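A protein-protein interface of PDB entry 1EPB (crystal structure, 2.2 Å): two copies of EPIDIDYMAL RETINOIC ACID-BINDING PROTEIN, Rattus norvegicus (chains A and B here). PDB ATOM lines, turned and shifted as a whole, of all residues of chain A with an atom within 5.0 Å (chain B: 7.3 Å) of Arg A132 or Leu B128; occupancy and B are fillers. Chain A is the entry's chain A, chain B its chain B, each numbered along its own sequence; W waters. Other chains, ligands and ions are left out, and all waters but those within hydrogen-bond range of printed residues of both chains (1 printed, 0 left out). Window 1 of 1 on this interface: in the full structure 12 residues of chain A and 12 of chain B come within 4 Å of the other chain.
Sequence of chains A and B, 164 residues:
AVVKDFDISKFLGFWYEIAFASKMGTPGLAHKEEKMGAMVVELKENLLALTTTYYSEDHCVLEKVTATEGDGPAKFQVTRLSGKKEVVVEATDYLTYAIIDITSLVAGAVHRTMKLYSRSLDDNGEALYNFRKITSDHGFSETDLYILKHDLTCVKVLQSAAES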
ATOM      1  N   LEU A 128      23.153  27.481 -21.927  1.00  0.00           N
ATOM      2  CA  LEU A 128      23.577  26.486 -20.983  1.00  0.00           C
ATOM      3  C   LEU A 128      23.651  25.104 -21.605  1.00  0.00           C
ATOM      4  O   LEU A 128      24.633  24.403 -21.360  1.00  0.00           O
ATOM      5  CB  LEU A 128      22.654  26.489 -19.759  1.00  0.00           C
ATOM      6  CG  LEU A 128      23.061  27.587 -18.732  1.00  0.00           C
ATOM      7  CD1 LEU A 128      21.872  27.948 -17.867  1.00  0.00           C
ATOM      8  CD2 LEU A 128      24.307  27.078 -17.927  1.00  0.00           C
ATOM      9  N   TYR A 129      22.741  24.794 -22.514  1.00  0.00           N
ATOM     10  CA  TYR A 129      22.786  23.512 -23.184  1.00  0.00           C
ATOM     11  C   TYR A 129      23.996  23.390 -24.111  1.00  0.00           C
ATOM     12  O   TYR A 129      24.664  22.345 -24.143  1.00  0.00           O
ATOM     13  CB  TYR A 129      21.489  23.313 -23.942  1.00  0.00           C
ATOM     14  CG  TYR A 129      21.337  21.953 -24.622  1.00  0.00           C
ATOM     15  CD1 TYR A 129      21.511  20.742 -23.964  1.00  0.00           C
ATOM     16  CD2 TYR A 129      20.956  21.993 -25.949  1.00  0.00           C
ATOM     17  CE1 TYR A 129      21.277  19.577 -24.649  1.00  0.00           C
ATOM     18  CE2 TYR A 129      20.728  20.829 -26.643  1.00  0.00           C
ATOM     19  CZ  TYR A 129      20.880  19.633 -25.979  1.00  0.00           C
ATOM     20  OH  TYR A 129      20.541  18.501 -26.704  1.00  0.00           O
ATOM     21  N   ASN A 130      24.299  24.441 -24.822  1.00  0.00           N
ATOM     22  CA  ASN A 130      25.516  24.489 -25.630  1.00  0.00           C
ATOM     23  C   ASN A 130      26.782  24.392 -24.773  1.00  0.00           C
ATOM     24  O   ASN A 130      27.752  23.725 -25.179  1.00  0.00           O
ATOM     25  CB  ASN A 130      25.650  25.789 -26.454  1.00  0.00           C
ATOM     26  CG  ASN A 130      24.660  25.873 -27.602  1.00  0.00           C
ATOM     27  OD1 ASN A 130      23.952  24.926 -27.936  1.00  0.00           O
ATOM     28  ND2 ASN A 130      24.526  27.013 -28.260  1.00  0.00           N
ATOM     29  N   PHE A 131      26.779  24.951 -23.557  1.00  0.00           N
ATOM     30  CA  PHE A 131      27.971  24.917 -22.719  1.00  0.00           C
ATOM     31  C   PHE A 131      28.254  23.465 -22.362  1.00  0.00           C
ATOM     32  O   PHE A 131      29.401  23.030 -22.548  1.00  0.00           O
ATOM     33  CB  PHE A 131      27.762  25.744 -21.463  1.00  0.00           C
ATOM     34  CG  PHE A 131      28.994  25.955 -20.572  1.00  0.00           C
ATOM     35  CD1 PHE A 131      30.109  26.623 -21.052  1.00  0.00           C
ATOM     36  CD2 PHE A 131      29.002  25.480 -19.269  1.00  0.00           C
ATOM     37  CE1 PHE A 131      31.193  26.806 -20.228  1.00  0.00           C
ATOM     38  CE2 PHE A 131      30.100  25.669 -18.461  1.00  0.00           C
ATOM     39  CZ  PHE A 131      31.195  26.329 -18.934  1.00  0.00           C
ATOM     40  N   ARG A 132      27.172  22.725 -22.044  1.00  0.00           N
ATOM     41  CA  ARG A 132      27.296  21.323 -21.656  1.00  0.00           C
ATOM     42  C   ARG A 132      27.812  20.499 -22.850  1.00  0.00           C
ATOM     43  O   ARG A 132      28.729  19.695 -22.623  1.00  0.00           O
ATOM     44  CB  ARG A 132      25.936  20.771 -21.156  1.00  0.00           C
ATOM     45  CG  ARG A 132      25.510  21.559 -19.947  1.00  0.00           C
ATOM     46  CD  ARG A 132      24.157  21.079 -19.460  1.00  0.00           C
ATOM     47  NE  ARG A 132      23.808  21.467 -18.092  1.00  0.00           N
ATOM     48  CZ  ARG A 132      24.461  21.124 -16.970  1.00  0.00           C
ATOM     49  NH1 ARG A 132      25.568  20.367 -16.941  1.00  0.00           N
ATOM     50  NH2 ARG A 132      23.937  21.512 -15.813  1.00  0.00           N
ATOM     51  N   LYS A 133      27.360  20.756 -24.102  1.00  0.00           N
ATOM     52  CA  LYS A 133      27.919  20.047 -25.277  1.00  0.00           C
ATOM     53  C   LYS A 133      29.402  20.399 -25.526  1.00  0.00           C
ATOM     54  O   LYS A 133      30.312  19.548 -25.689  1.00  0.00           O
ATOM     55  CB  LYS A 133      27.115  20.353 -26.609  1.00  0.00           C
ATOM     56  CG  LYS A 133      25.640  19.851 -26.559  1.00  0.00           C
ATOM     57  CD  LYS A 133      24.678  20.393 -27.641  1.00  0.00           C
ATOM     58  CE  LYS A 133      24.903  19.830 -29.078  1.00  0.00           C
ATOM     59  NZ  LYS A 133      24.178  20.511 -30.151  1.00  0.00           N
ATOM     60  N   ILE A 134      29.693  21.687 -25.475  1.00  0.00           N
ATOM     61  CA  ILE A 134      31.049  22.055 -25.778  1.00  0.00           C
ATOM     62  C   ILE A 134      31.994  21.569 -24.687  1.00  0.00           C
ATOM     63  O   ILE A 134      33.068  21.088 -25.034  1.00  0.00           O
ATOM     64  CB  ILE A 134      31.068  23.618 -26.000  1.00  0.00           C
ATOM     65  CG1 ILE A 134      30.681  23.897 -27.482  1.00  0.00           C
ATOM     66  CG2 ILE A 134      32.444  24.244 -25.713  1.00  0.00           C
ATOM     67  CD1 ILE A 134      29.926  25.229 -27.792  1.00  0.00           C
ATOM     68  N   THR A 135      31.691  21.638 -23.391  1.00  0.00           N
ATOM     69  CA  THR A 135      32.647  21.267 -22.397  1.00  0.00           C
ATOM     70  C   THR A 135      32.798  19.764 -22.380  1.00  0.00           C
ATOM     71  O   THR A 135      33.917  19.343 -22.075  1.00  0.00           O
ATOM     72  CB  THR A 135      32.262  21.750 -20.984  1.00  0.00           C
ATOM     73  OG1 THR A 135      30.978  21.196 -20.672  1.00  0.00           O
ATOM     74  CG2 THR A 135      32.359  23.297 -20.873  1.00  0.00           C
ATOM     75  N   SER A 136      31.783  18.973 -22.755  1.00  0.00           N
ATOM     76  CA  SER A 136      31.990  17.541 -22.769  1.00  0.00           C
ATOM     77  C   SER A 136      32.953  17.290 -23.915  1.00  0.00           C
ATOM     78  O   SER A 136      33.873  16.495 -23.710  1.00  0.00           O
ATOM     79  CB  SER A 136      30.683  16.703 -22.985  1.00  0.00           C
ATOM     80  OG  SER A 136      29.950  16.835 -24.194  1.00  0.00           O
ATOM     81  N   GLU A 142      30.108  16.271 -16.549  1.00  0.00           N
ATOM     82  CA  GLU A 142      28.982  16.942 -15.859  1.00  0.00           C
ATOM     83  C   GLU A 142      29.284  17.341 -14.416  1.00  0.00           C
ATOM     84  O   GLU A 142      28.787  18.330 -13.879  1.00  0.00           O
ATOM     85  CB  GLU A 142      27.743  16.054 -15.806  1.00  0.00           C
ATOM     86  CG  GLU A 142      26.475  16.836 -15.397  1.00  0.00           C
ATOM     87  CD  GLU A 142      25.222  15.959 -15.439  1.00  0.00           C
ATOM     88  OE1 GLU A 142      24.980  15.295 -16.445  1.00  0.00           O
ATOM     89  OE2 GLU A 142      24.488  15.932 -14.454  1.00  0.00           O
ATOM     90  N   LEU A 145      30.993  20.841 -13.986  1.00  0.00           N
ATOM     91  CA  LEU A 145      30.360  22.111 -14.321  1.00  0.00           C
ATOM     92  C   LEU A 145      29.713  22.734 -13.089  1.00  0.00           C
ATOM     93  O   LEU A 145      29.009  22.052 -12.318  1.00  0.00           O
ATOM     94  CB  LEU A 145      29.289  21.909 -15.410  1.00  0.00           C
ATOM     95  CG  LEU A 145      29.501  21.115 -16.716  1.00  0.00           C
ATOM     96  CD1 LEU A 145      28.497  21.584 -17.800  1.00  0.00           C
ATOM     97  CD2 LEU A 145      30.937  21.295 -17.207  1.00  0.00           C
ATOM     98  N   ILE A 147      27.148  25.749 -11.933  1.00  0.00           N
ATOM     99  CA  ILE A 147      26.141  26.750 -12.311  1.00  0.00           C
ATOM    100  C   ILE A 147      26.100  27.744 -11.116  1.00  0.00           C
ATOM    101  O   ILE A 147      25.847  27.383  -9.970  1.00  0.00           O
ATOM    102  CB  ILE A 147      24.702  26.088 -12.554  1.00  0.00           C
ATOM    103  CG1 ILE A 147      24.687  25.219 -13.815  1.00  0.00           C
ATOM    104  CG2 ILE A 147      23.632  27.186 -12.740  1.00  0.00           C
ATOM    105  CD1 ILE A 147      25.337  23.832 -13.722  1.00  0.00           C
ATOM    106  N   ILE B  18      18.543  15.242  -9.633  1.00  0.00           N
ATOM    107  CA  ILE B  18      19.456  16.111 -10.377  1.00  0.00           C
ATOM    108  C   ILE B  18      19.215  17.624 -10.248  1.00  0.00           C
ATOM    109  O   ILE B  18      20.165  18.432 -10.277  1.00  0.00           O
ATOM    110  CB  ILE B  18      19.398  15.597 -11.873  1.00  0.00           C
ATOM    111  CG1 ILE B  18      19.955  14.134 -11.884  1.00  0.00           C
ATOM    112  CG2 ILE B  18      20.186  16.517 -12.857  1.00  0.00           C
ATOM    113  CD1 ILE B  18      21.417  14.015 -11.393  1.00  0.00           C
ATOM    114  N   ALA B  19      17.922  17.973 -10.106  1.00  0.00           N
ATOM    115  CA  ALA B  19      17.471  19.344  -9.985  1.00  0.00           C
ATOM    116  C   ALA B  19      16.080  19.354  -9.369  1.00  0.00           C
ATOM    117  O   ALA B  19      15.427  18.294  -9.313  1.00  0.00           O
ATOM    118  CB  ALA B  19      17.384  20.023 -11.363  1.00  0.00           C
ATOM    119  N   TYR B  97      15.326   9.311 -17.484  1.00  0.00           N
ATOM    120  CA  TYR B  97      14.942  10.395 -16.636  1.00  0.00           C
ATOM    121  C   TYR B  97      13.422  10.439 -16.479  1.00  0.00           C
ATOM    122  O   TYR B  97      12.695   9.816 -17.274  1.00  0.00           O
ATOM    123  CB  TYR B  97      15.467  11.745 -17.208  1.00  0.00           C
ATOM    124  CG  TYR B  97      14.666  12.409 -18.331  1.00  0.00           C
ATOM    125  CD1 TYR B  97      13.628  13.312 -18.098  1.00  0.00           C
ATOM    126  CD2 TYR B  97      14.976  12.085 -19.606  1.00  0.00           C
ATOM    127  CE1 TYR B  97      12.920  13.860 -19.150  1.00  0.00           C
ATOM    128  CE2 TYR B  97      14.289  12.615 -20.657  1.00  0.00           C
ATOM    129  CZ  TYR B  97      13.253  13.494 -20.445  1.00  0.00           C
ATOM    130  OH  TYR B  97      12.514  13.914 -21.562  1.00  0.00           O
ATOM    131  N   ILE B  99      10.546  13.738 -15.095  1.00  0.00           N
ATOM    132  CA  ILE B  99      10.225  15.034 -14.472  1.00  0.00           C
ATOM    133  C   ILE B  99       8.874  14.912 -13.734  1.00  0.00           C
ATOM    134  O   ILE B  99       7.829  14.599 -14.317  1.00  0.00           O
ATOM    135  CB  ILE B  99      10.166  16.179 -15.556  1.00  0.00           C
ATOM    136  CG1 ILE B  99      11.570  16.375 -16.176  1.00  0.00           C
ATOM    137  CG2 ILE B  99       9.673  17.493 -14.912  1.00  0.00           C
ATOM    138  CD1 ILE B  99      11.657  17.385 -17.349  1.00  0.00           C
ATOM    139  N   LEU B 116      13.605  16.741 -11.069  1.00  0.00           N
ATOM    140  CA  LEU B 116      14.147  15.958 -12.147  1.00  0.00           C
ATOM    141  C   LEU B 116      14.922  14.783 -11.546  1.00  0.00           C
ATOM    142  O   LEU B 116      15.910  14.943 -10.786  1.00  0.00           O
ATOM    143  CB  LEU B 116      15.093  16.833 -13.036  1.00  0.00           C
ATOM    144  CG  LEU B 116      16.062  16.166 -14.032  1.00  0.00           C
ATOM    145  CD1 LEU B 116      15.235  15.423 -15.057  1.00  0.00           C
ATOM    146  CD2 LEU B 116      16.957  17.204 -14.762  1.00  0.00           C
ATOM    147  N   ASP B 123      25.701  13.013 -18.716  1.00  0.00           N
ATOM    148  CA  ASP B 123      24.830  13.117 -19.885  1.00  0.00           C
ATOM    149  C   ASP B 123      23.363  13.495 -19.627  1.00  0.00           C
ATOM    150  O   ASP B 123      22.439  13.097 -20.374  1.00  0.00           O
ATOM    151  CB  ASP B 123      24.876  11.777 -20.699  1.00  0.00           C
ATOM    152  CG  ASP B 123      24.642  11.872 -22.219  1.00  0.00           C
ATOM    153  OD1 ASP B 123      24.464  12.983 -22.752  1.00  0.00           O
ATOM    154  OD2 ASP B 123      24.641  10.815 -22.869  1.00  0.00           O
ATOM    155  N   ASN B 124      23.219  14.408 -18.636  1.00  0.00           N
ATOM    156  CA  ASN B 124      21.882  14.884 -18.256  1.00  0.00           C
ATOM    157  C   ASN B 124      21.451  16.104 -19.041  1.00  0.00           C
ATOM    158  O   ASN B 124      20.400  16.659 -18.770  1.00  0.00           O
ATOM    159  CB  ASN B 124      21.794  15.234 -16.749  1.00  0.00           C
ATOM    160  CG  ASN B 124      21.833  13.977 -15.910  1.00  0.00           C
ATOM    161  OD1 ASN B 124      21.077  13.057 -16.188  1.00  0.00           O
ATOM    162  ND2 ASN B 124      22.604  13.807 -14.840  1.00  0.00           N
ATOM    163  N   GLY B 125      22.215  16.461 -20.082  1.00  0.00           N
ATOM    164  CA  GLY B 125      22.064  17.644 -20.943  1.00  0.00           C
ATOM    165  C   GLY B 125      20.643  17.922 -21.442  1.00  0.00           C
ATOM    166  O   GLY B 125      20.008  18.918 -21.093  1.00  0.00           O
ATOM    167  N   GLU B 126      20.146  16.955 -22.193  1.00  0.00           N
ATOM    168  CA  GLU B 126      18.836  17.036 -22.799  1.00  0.00           C
ATOM    169  C   GLU B 126      17.731  17.008 -21.714  1.00  0.00           C
ATOM    170  O   GLU B 126      16.776  17.782 -21.783  1.00  0.00           O
ATOM    171  CB  GLU B 126      18.755  15.866 -23.825  1.00  0.00           C
ATOM    172  CG  GLU B 126      19.804  15.820 -25.012  1.00  0.00           C
ATOM    173  CD  GLU B 126      21.342  15.673 -24.723  1.00  0.00           C
ATOM    174  OE1 GLU B 126      21.745  14.964 -23.772  1.00  0.00           O
ATOM    175  OE2 GLU B 126      22.150  16.269 -25.457  1.00  0.00           O
ATOM    176  N   ALA B 127      17.865  16.229 -20.635  1.00  0.00           N
ATOM    177  CA  ALA B 127      16.859  16.159 -19.549  1.00  0.00           C
ATOM    178  C   ALA B 127      16.803  17.543 -18.894  1.00  0.00           C
ATOM    179  O   ALA B 127      15.726  18.128 -18.736  1.00  0.00           O
ATOM    180  CB  ALA B 127      17.236  15.144 -18.426  1.00  0.00           C
ATOM    181  N   LEU B 128      17.976  18.107 -18.638  1.00  0.00           N
ATOM    182  CA  LEU B 128      18.041  19.414 -18.010  1.00  0.00           C
ATOM    183  C   LEU B 128      17.441  20.511 -18.859  1.00  0.00           C
ATOM    184  O   LEU B 128      16.774  21.430 -18.361  1.00  0.00           O
ATOM    185  CB  LEU B 128      19.470  19.724 -17.688  1.00  0.00           C
ATOM    186  CG  LEU B 128      19.978  19.020 -16.392  1.00  0.00           C
ATOM    187  CD1 LEU B 128      21.532  18.915 -16.419  1.00  0.00           C
ATOM    188  CD2 LEU B 128      19.473  19.803 -15.173  1.00  0.00           C
ATOM    189  N   TYR B 129      17.626  20.353 -20.168  1.00  0.00           N
ATOM    190  CA  TYR B 129      17.099  21.286 -21.141  1.00  0.00           C
ATOM    191  C   TYR B 129      15.550  21.304 -21.070  1.00  0.00           C
ATOM    192  O   TYR B 129      14.885  22.365 -20.989  1.00  0.00           O
ATOM    193  CB  TYR B 129      17.609  20.851 -22.538  1.00  0.00           C
ATOM    194  CG  TYR B 129      17.267  21.893 -23.578  1.00  0.00           C
ATOM    195  CD1 TYR B 129      17.605  23.247 -23.365  1.00  0.00           C
ATOM    196  CD2 TYR B 129      16.627  21.471 -24.731  1.00  0.00           C
ATOM    197  CE1 TYR B 129      17.303  24.203 -24.324  1.00  0.00           C
ATOM    198  CE2 TYR B 129      16.323  22.431 -25.678  1.00  0.00           C
ATOM    199  CZ  TYR B 129      16.662  23.762 -25.473  1.00  0.00           C
ATOM    200  OH  TYR B 129      16.354  24.648 -26.477  1.00  0.00           O
ATOM    201  N   ASN B 130      14.999  20.082 -21.069  1.00  0.00           N
ATOM    202  CA  ASN B 130      13.565  19.908 -20.972  1.00  0.00           C
ATOM    203  C   ASN B 130      13.027  20.489 -19.677  1.00  0.00           C
ATOM    204  O   ASN B 130      11.993  21.183 -19.690  1.00  0.00           O
ATOM    205  CB  ASN B 130      13.124  18.453 -20.979  1.00  0.00           C
ATOM    206  CG  ASN B 130      13.383  17.801 -22.304  1.00  0.00           C
ATOM    207  OD1 ASN B 130      13.635  18.442 -23.324  1.00  0.00           O
ATOM    208  ND2 ASN B 130      13.378  16.483 -22.352  1.00  0.00           N
ATOM    209  N   PHE B 131      13.777  20.221 -18.586  1.00  0.00           N
ATOM    210  CA  PHE B 131      13.332  20.572 -17.278  1.00  0.00           C
ATOM    211  C   PHE B 131      13.224  22.080 -17.258  1.00  0.00           C
ATOM    212  O   PHE B 131      12.178  22.578 -16.829  1.00  0.00           O
ATOM    213  CB  PHE B 131      14.308  20.121 -16.223  1.00  0.00           C
ATOM    214  CG  PHE B 131      13.795  20.292 -14.796  1.00  0.00           C
ATOM    215  CD1 PHE B 131      12.643  19.617 -14.371  1.00  0.00           C
ATOM    216  CD2 PHE B 131      14.469  21.115 -13.893  1.00  0.00           C
ATOM    217  CE1 PHE B 131      12.203  19.777 -13.054  1.00  0.00           C
ATOM    218  CE2 PHE B 131      14.007  21.257 -12.579  1.00  0.00           C
ATOM    219  CZ  PHE B 131      12.875  20.590 -12.164  1.00  0.00           C
ATOM    220  N   ARG B 132      14.241  22.780 -17.773  1.00  0.00           N
ATOM    221  CA  ARG B 132      14.176  24.235 -17.845  1.00  0.00           C
ATOM    222  C   ARG B 132      12.990  24.650 -18.701  1.00  0.00           C
ATOM    223  O   ARG B 132      12.271  25.548 -18.240  1.00  0.00           O
ATOM    224  CB  ARG B 132      15.428  24.886 -18.457  1.00  0.00           C
ATOM    225  CG  ARG B 132      16.627  24.815 -17.562  1.00  0.00           C
ATOM    226  CD  ARG B 132      17.933  25.464 -18.061  1.00  0.00           C
ATOM    227  NE  ARG B 132      18.613  25.981 -16.867  1.00  0.00           N
ATOM    228  CZ  ARG B 132      19.682  25.421 -16.276  1.00  0.00           C
ATOM    229  NH1 ARG B 132      20.308  24.282 -16.732  1.00  0.00           N
ATOM    230  NH2 ARG B 132      20.079  26.008 -15.135  1.00  0.00           N
ATOM    231  N   LYS B 133      12.672  24.021 -19.842  1.00  0.00           N
ATOM    232  CA  LYS B 133      11.482  24.460 -20.587  1.00  0.00           C
ATOM    233  C   LYS B 133      10.151  24.252 -19.852  1.00  0.00           C
ATOM    234  O   LYS B 133       9.336  25.178 -19.771  1.00  0.00           O
ATOM    235  CB  LYS B 133      11.362  23.754 -21.939  1.00  0.00           C
ATOM    236  CG  LYS B 133      12.528  24.043 -22.871  1.00  0.00           C
ATOM    237  CD  LYS B 133      12.362  23.481 -24.280  1.00  0.00           C
ATOM    238  CE  LYS B 133      12.205  21.958 -24.322  1.00  0.00           C
ATOM    239  NZ  LYS B 133      11.890  21.499 -25.673  1.00  0.00           N
ATOM    240  N   ILE B 134       9.902  23.075 -19.287  1.00  0.00           N
ATOM    241  CA  ILE B 134       8.675  22.760 -18.527  1.00  0.00           C
ATOM    242  C   ILE B 134       8.541  23.654 -17.271  1.00  0.00           C
ATOM    243  O   ILE B 134       7.422  24.160 -17.028  1.00  0.00           O
ATOM    244  CB  ILE B 134       8.650  21.241 -18.067  1.00  0.00           C
ATOM    245  CG1 ILE B 134       8.506  20.403 -19.288  1.00  0.00           C
ATOM    246  CG2 ILE B 134       7.503  20.921 -17.107  1.00  0.00           C
ATOM    247  CD1 ILE B 134       8.723  18.906 -19.047  1.00  0.00           C
ATOM    248  N   THR B 135       9.630  23.850 -16.479  1.00  0.00           N
ATOM    249  CA  THR B 135       9.504  24.634 -15.249  1.00  0.00           C
ATOM    250  C   THR B 135       9.157  26.056 -15.658  1.00  0.00           C
ATOM    251  O   THR B 135       8.345  26.682 -14.986  1.00  0.00           O
ATOM    252  CB  THR B 135      10.784  24.719 -14.327  1.00  0.00           C
ATOM    253  OG1 THR B 135      11.909  25.117 -15.125  1.00  0.00           O
ATOM    254  CG2 THR B 135      11.008  23.400 -13.578  1.00  0.00           C
ATOM    255  N   LEU B 145      15.273  27.513  -9.975  1.00  0.00           N
ATOM    256  CA  LEU B 145      15.752  26.185 -10.248  1.00  0.00           C
ATOM    257  C   LEU B 145      16.953  26.001  -9.366  1.00  0.00           C
ATOM    258  O   LEU B 145      17.741  26.920  -9.111  1.00  0.00           O
ATOM    259  CB  LEU B 145      16.186  25.999 -11.696  1.00  0.00           C
ATOM    260  CG  LEU B 145      15.457  26.632 -12.874  1.00  0.00           C
ATOM    261  CD1 LEU B 145      15.793  25.780 -14.104  1.00  0.00           C
ATOM    262  CD2 LEU B 145      13.948  26.696 -12.657  1.00  0.00           C
ATOM    263  N   TYR B 146      17.114  24.764  -8.966  1.00  0.00           N
ATOM    264  CA  TYR B 146      18.192  24.300  -8.097  1.00  0.00           C
ATOM    265  C   TYR B 146      18.840  23.086  -8.717  1.00  0.00           C
ATOM    266  O   TYR B 146      18.247  21.994  -8.667  1.00  0.00           O
ATOM    267  CB  TYR B 146      17.602  23.938  -6.733  1.00  0.00           C
ATOM    268  CG  TYR B 146      17.031  25.181  -6.068  1.00  0.00           C
ATOM    269  CD1 TYR B 146      17.883  25.976  -5.330  1.00  0.00           C
ATOM    270  CD2 TYR B 146      15.706  25.521  -6.255  1.00  0.00           C
ATOM    271  CE1 TYR B 146      17.397  27.140  -4.779  1.00  0.00           C
ATOM    272  CE2 TYR B 146      15.214  26.677  -5.708  1.00  0.00           C
ATOM    273  CZ  TYR B 146      16.071  27.478  -4.974  1.00  0.00           C
ATOM    274  OH  TYR B 146      15.604  28.644  -4.403  1.00  0.00           O
ATOM    275  N   ILE B 147      20.016  23.262  -9.328  1.00  0.00           N
ATOM    276  CA  ILE B 147      20.754  22.144  -9.947  1.00  0.00           C
ATOM    277  C   ILE B 147      21.609  21.567  -8.837  1.00  0.00           C
ATOM    278  O   ILE B 147      22.556  22.237  -8.432  1.00  0.00           O
ATOM    279  CB  ILE B 147      21.687  22.630 -11.127  1.00  0.00           C
ATOM    280  CG1 ILE B 147      20.967  23.639 -12.021  1.00  0.00           C
ATOM    281  CG2 ILE B 147      22.115  21.463 -11.968  1.00  0.00           C
ATOM    282  CD1 ILE B 147      19.622  23.261 -12.705  1.00  0.00           C
ATOM    283  N   LEU B 148      21.365  20.358  -8.359  1.00  0.00           N
ATOM    284  CA  LEU B 148      22.045  19.787  -7.204  1.00  0.00           C
ATOM    285  C   LEU B 148      23.550  19.533  -7.317  1.00  0.00           C
ATOM    286  O   LEU B 148      24.050  19.087  -8.374  1.00  0.00           O
ATOM    287  CB  LEU B 148      21.349  18.476  -6.804  1.00  0.00           C
ATOM    288  CG  LEU B 148      20.117  18.702  -5.924  1.00  0.00           C
ATOM    289  CD1 LEU B 148      19.059  19.315  -6.762  1.00  0.00           C
ATOM    290  CD2 LEU B 148      19.618  17.409  -5.303  1.00  0.00           C
ATOM    291  N   HIS B 150      27.078  17.822  -6.855  1.00  0.00           N
ATOM    292  CA  HIS B 150      27.460  16.436  -6.956  1.00  0.00           C
ATOM    293  C   HIS B 150      28.214  15.921  -5.746  1.00  0.00           C
ATOM    294  O   HIS B 150      29.128  15.106  -5.883  1.00  0.00           O
ATOM    295  CB  HIS B 150      28.303  16.224  -8.238  1.00  0.00           C
ATOM    296  CG  HIS B 150      27.475  15.990  -9.504  1.00  0.00           C
ATOM    297  ND1 HIS B 150      27.577  14.996 -10.388  1.00  0.00           N
ATOM    298  CD2 HIS B 150      26.446  16.800  -9.920  1.00  0.00           C
ATOM    299  CE1 HIS B 150      26.660  15.164 -11.303  1.00  0.00           C
ATOM    300  NE2 HIS B 150      25.989  16.253 -11.010  1.00  0.00           N
HETATM  301  O   HOH W   1      24.124  17.826 -12.582  1.00  0.00           O
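Arg A132 touches just one residue of chain B: Leu B128 (3.6 Å). Of the printed residues of chain B, Tyr A129 touches Gly B125 (3.7 Å), Glu B126 (3.0 Å) and Tyr B129 (3.9 Å). Of the printed residues of chain A, His B150 touches Glu A142 (3.8 Å). Of the printed residues of chain B, Leu A128 touches Arg B132. Tyr B97 touches none of the printed residues of chain A. Ser A136 touches none of the printed residues of chain B.
The backbone carbonyl oxygen (O) of Arg A132 is in hydrogen-bond range of the side-chain hydroxyl (OG) of Ser A136. O of Arg A132 is in hydrogen-bond range of OG1 of Thr A135 (3.3 Å). The side-chain hydroxyl (OG1) of Thr B135 sits at hydrogen-bond distance from the backbone carbonyl oxygen (O) of Arg B132 (3.2 Å).
Water W1 bridges OE2 of Glu A142 (2.7 Å) and NE2 of His B150 (2.9 Å).
The backbone NH (N) of Asp B123 is in hydrogen-bond range of the side-chain carboxylate (OE1) of Glu A142, at 3.3 Å. OE2 of Glu B126 lies within hydrogen-bond range of OH of Tyr A129, at 3.0 Å. OE2 of Glu A142 lies within hydrogen-bond range of ND2 of Asn B124 (2.9 Å).
Of the 12 printed residues of chain A, 4 touch a printed residue of chain B. Printed residues of chain A that touch a printed residue of chain B: Leu A128, Tyr A129, Arg A132 and Glu A142. Of the 23 printed residues of chain B, 8 touch a printed residue of chain A. Among the printed residues, no Asp or Glu carboxylate lies within 4 Å of a Lys or Arg side-chain nitrogen of the other chain.
Among the printed residues, merely in contact across the chains: Arg A132 with Leu B128 (3.6 Å), Tyr A129 with Gly B125 (3.7 Å), Leu A128 with Arg B132 (3.7 Å), Glu A142 with His B150 (3.8 Å) and Tyr A129 with Tyr B129 (3.9 Å).
Leu A128 touches Arg B132, and with the chains exchanged Arg A132 touches Leu B128. Tyr A129 touches its own counterpart, Tyr B129.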
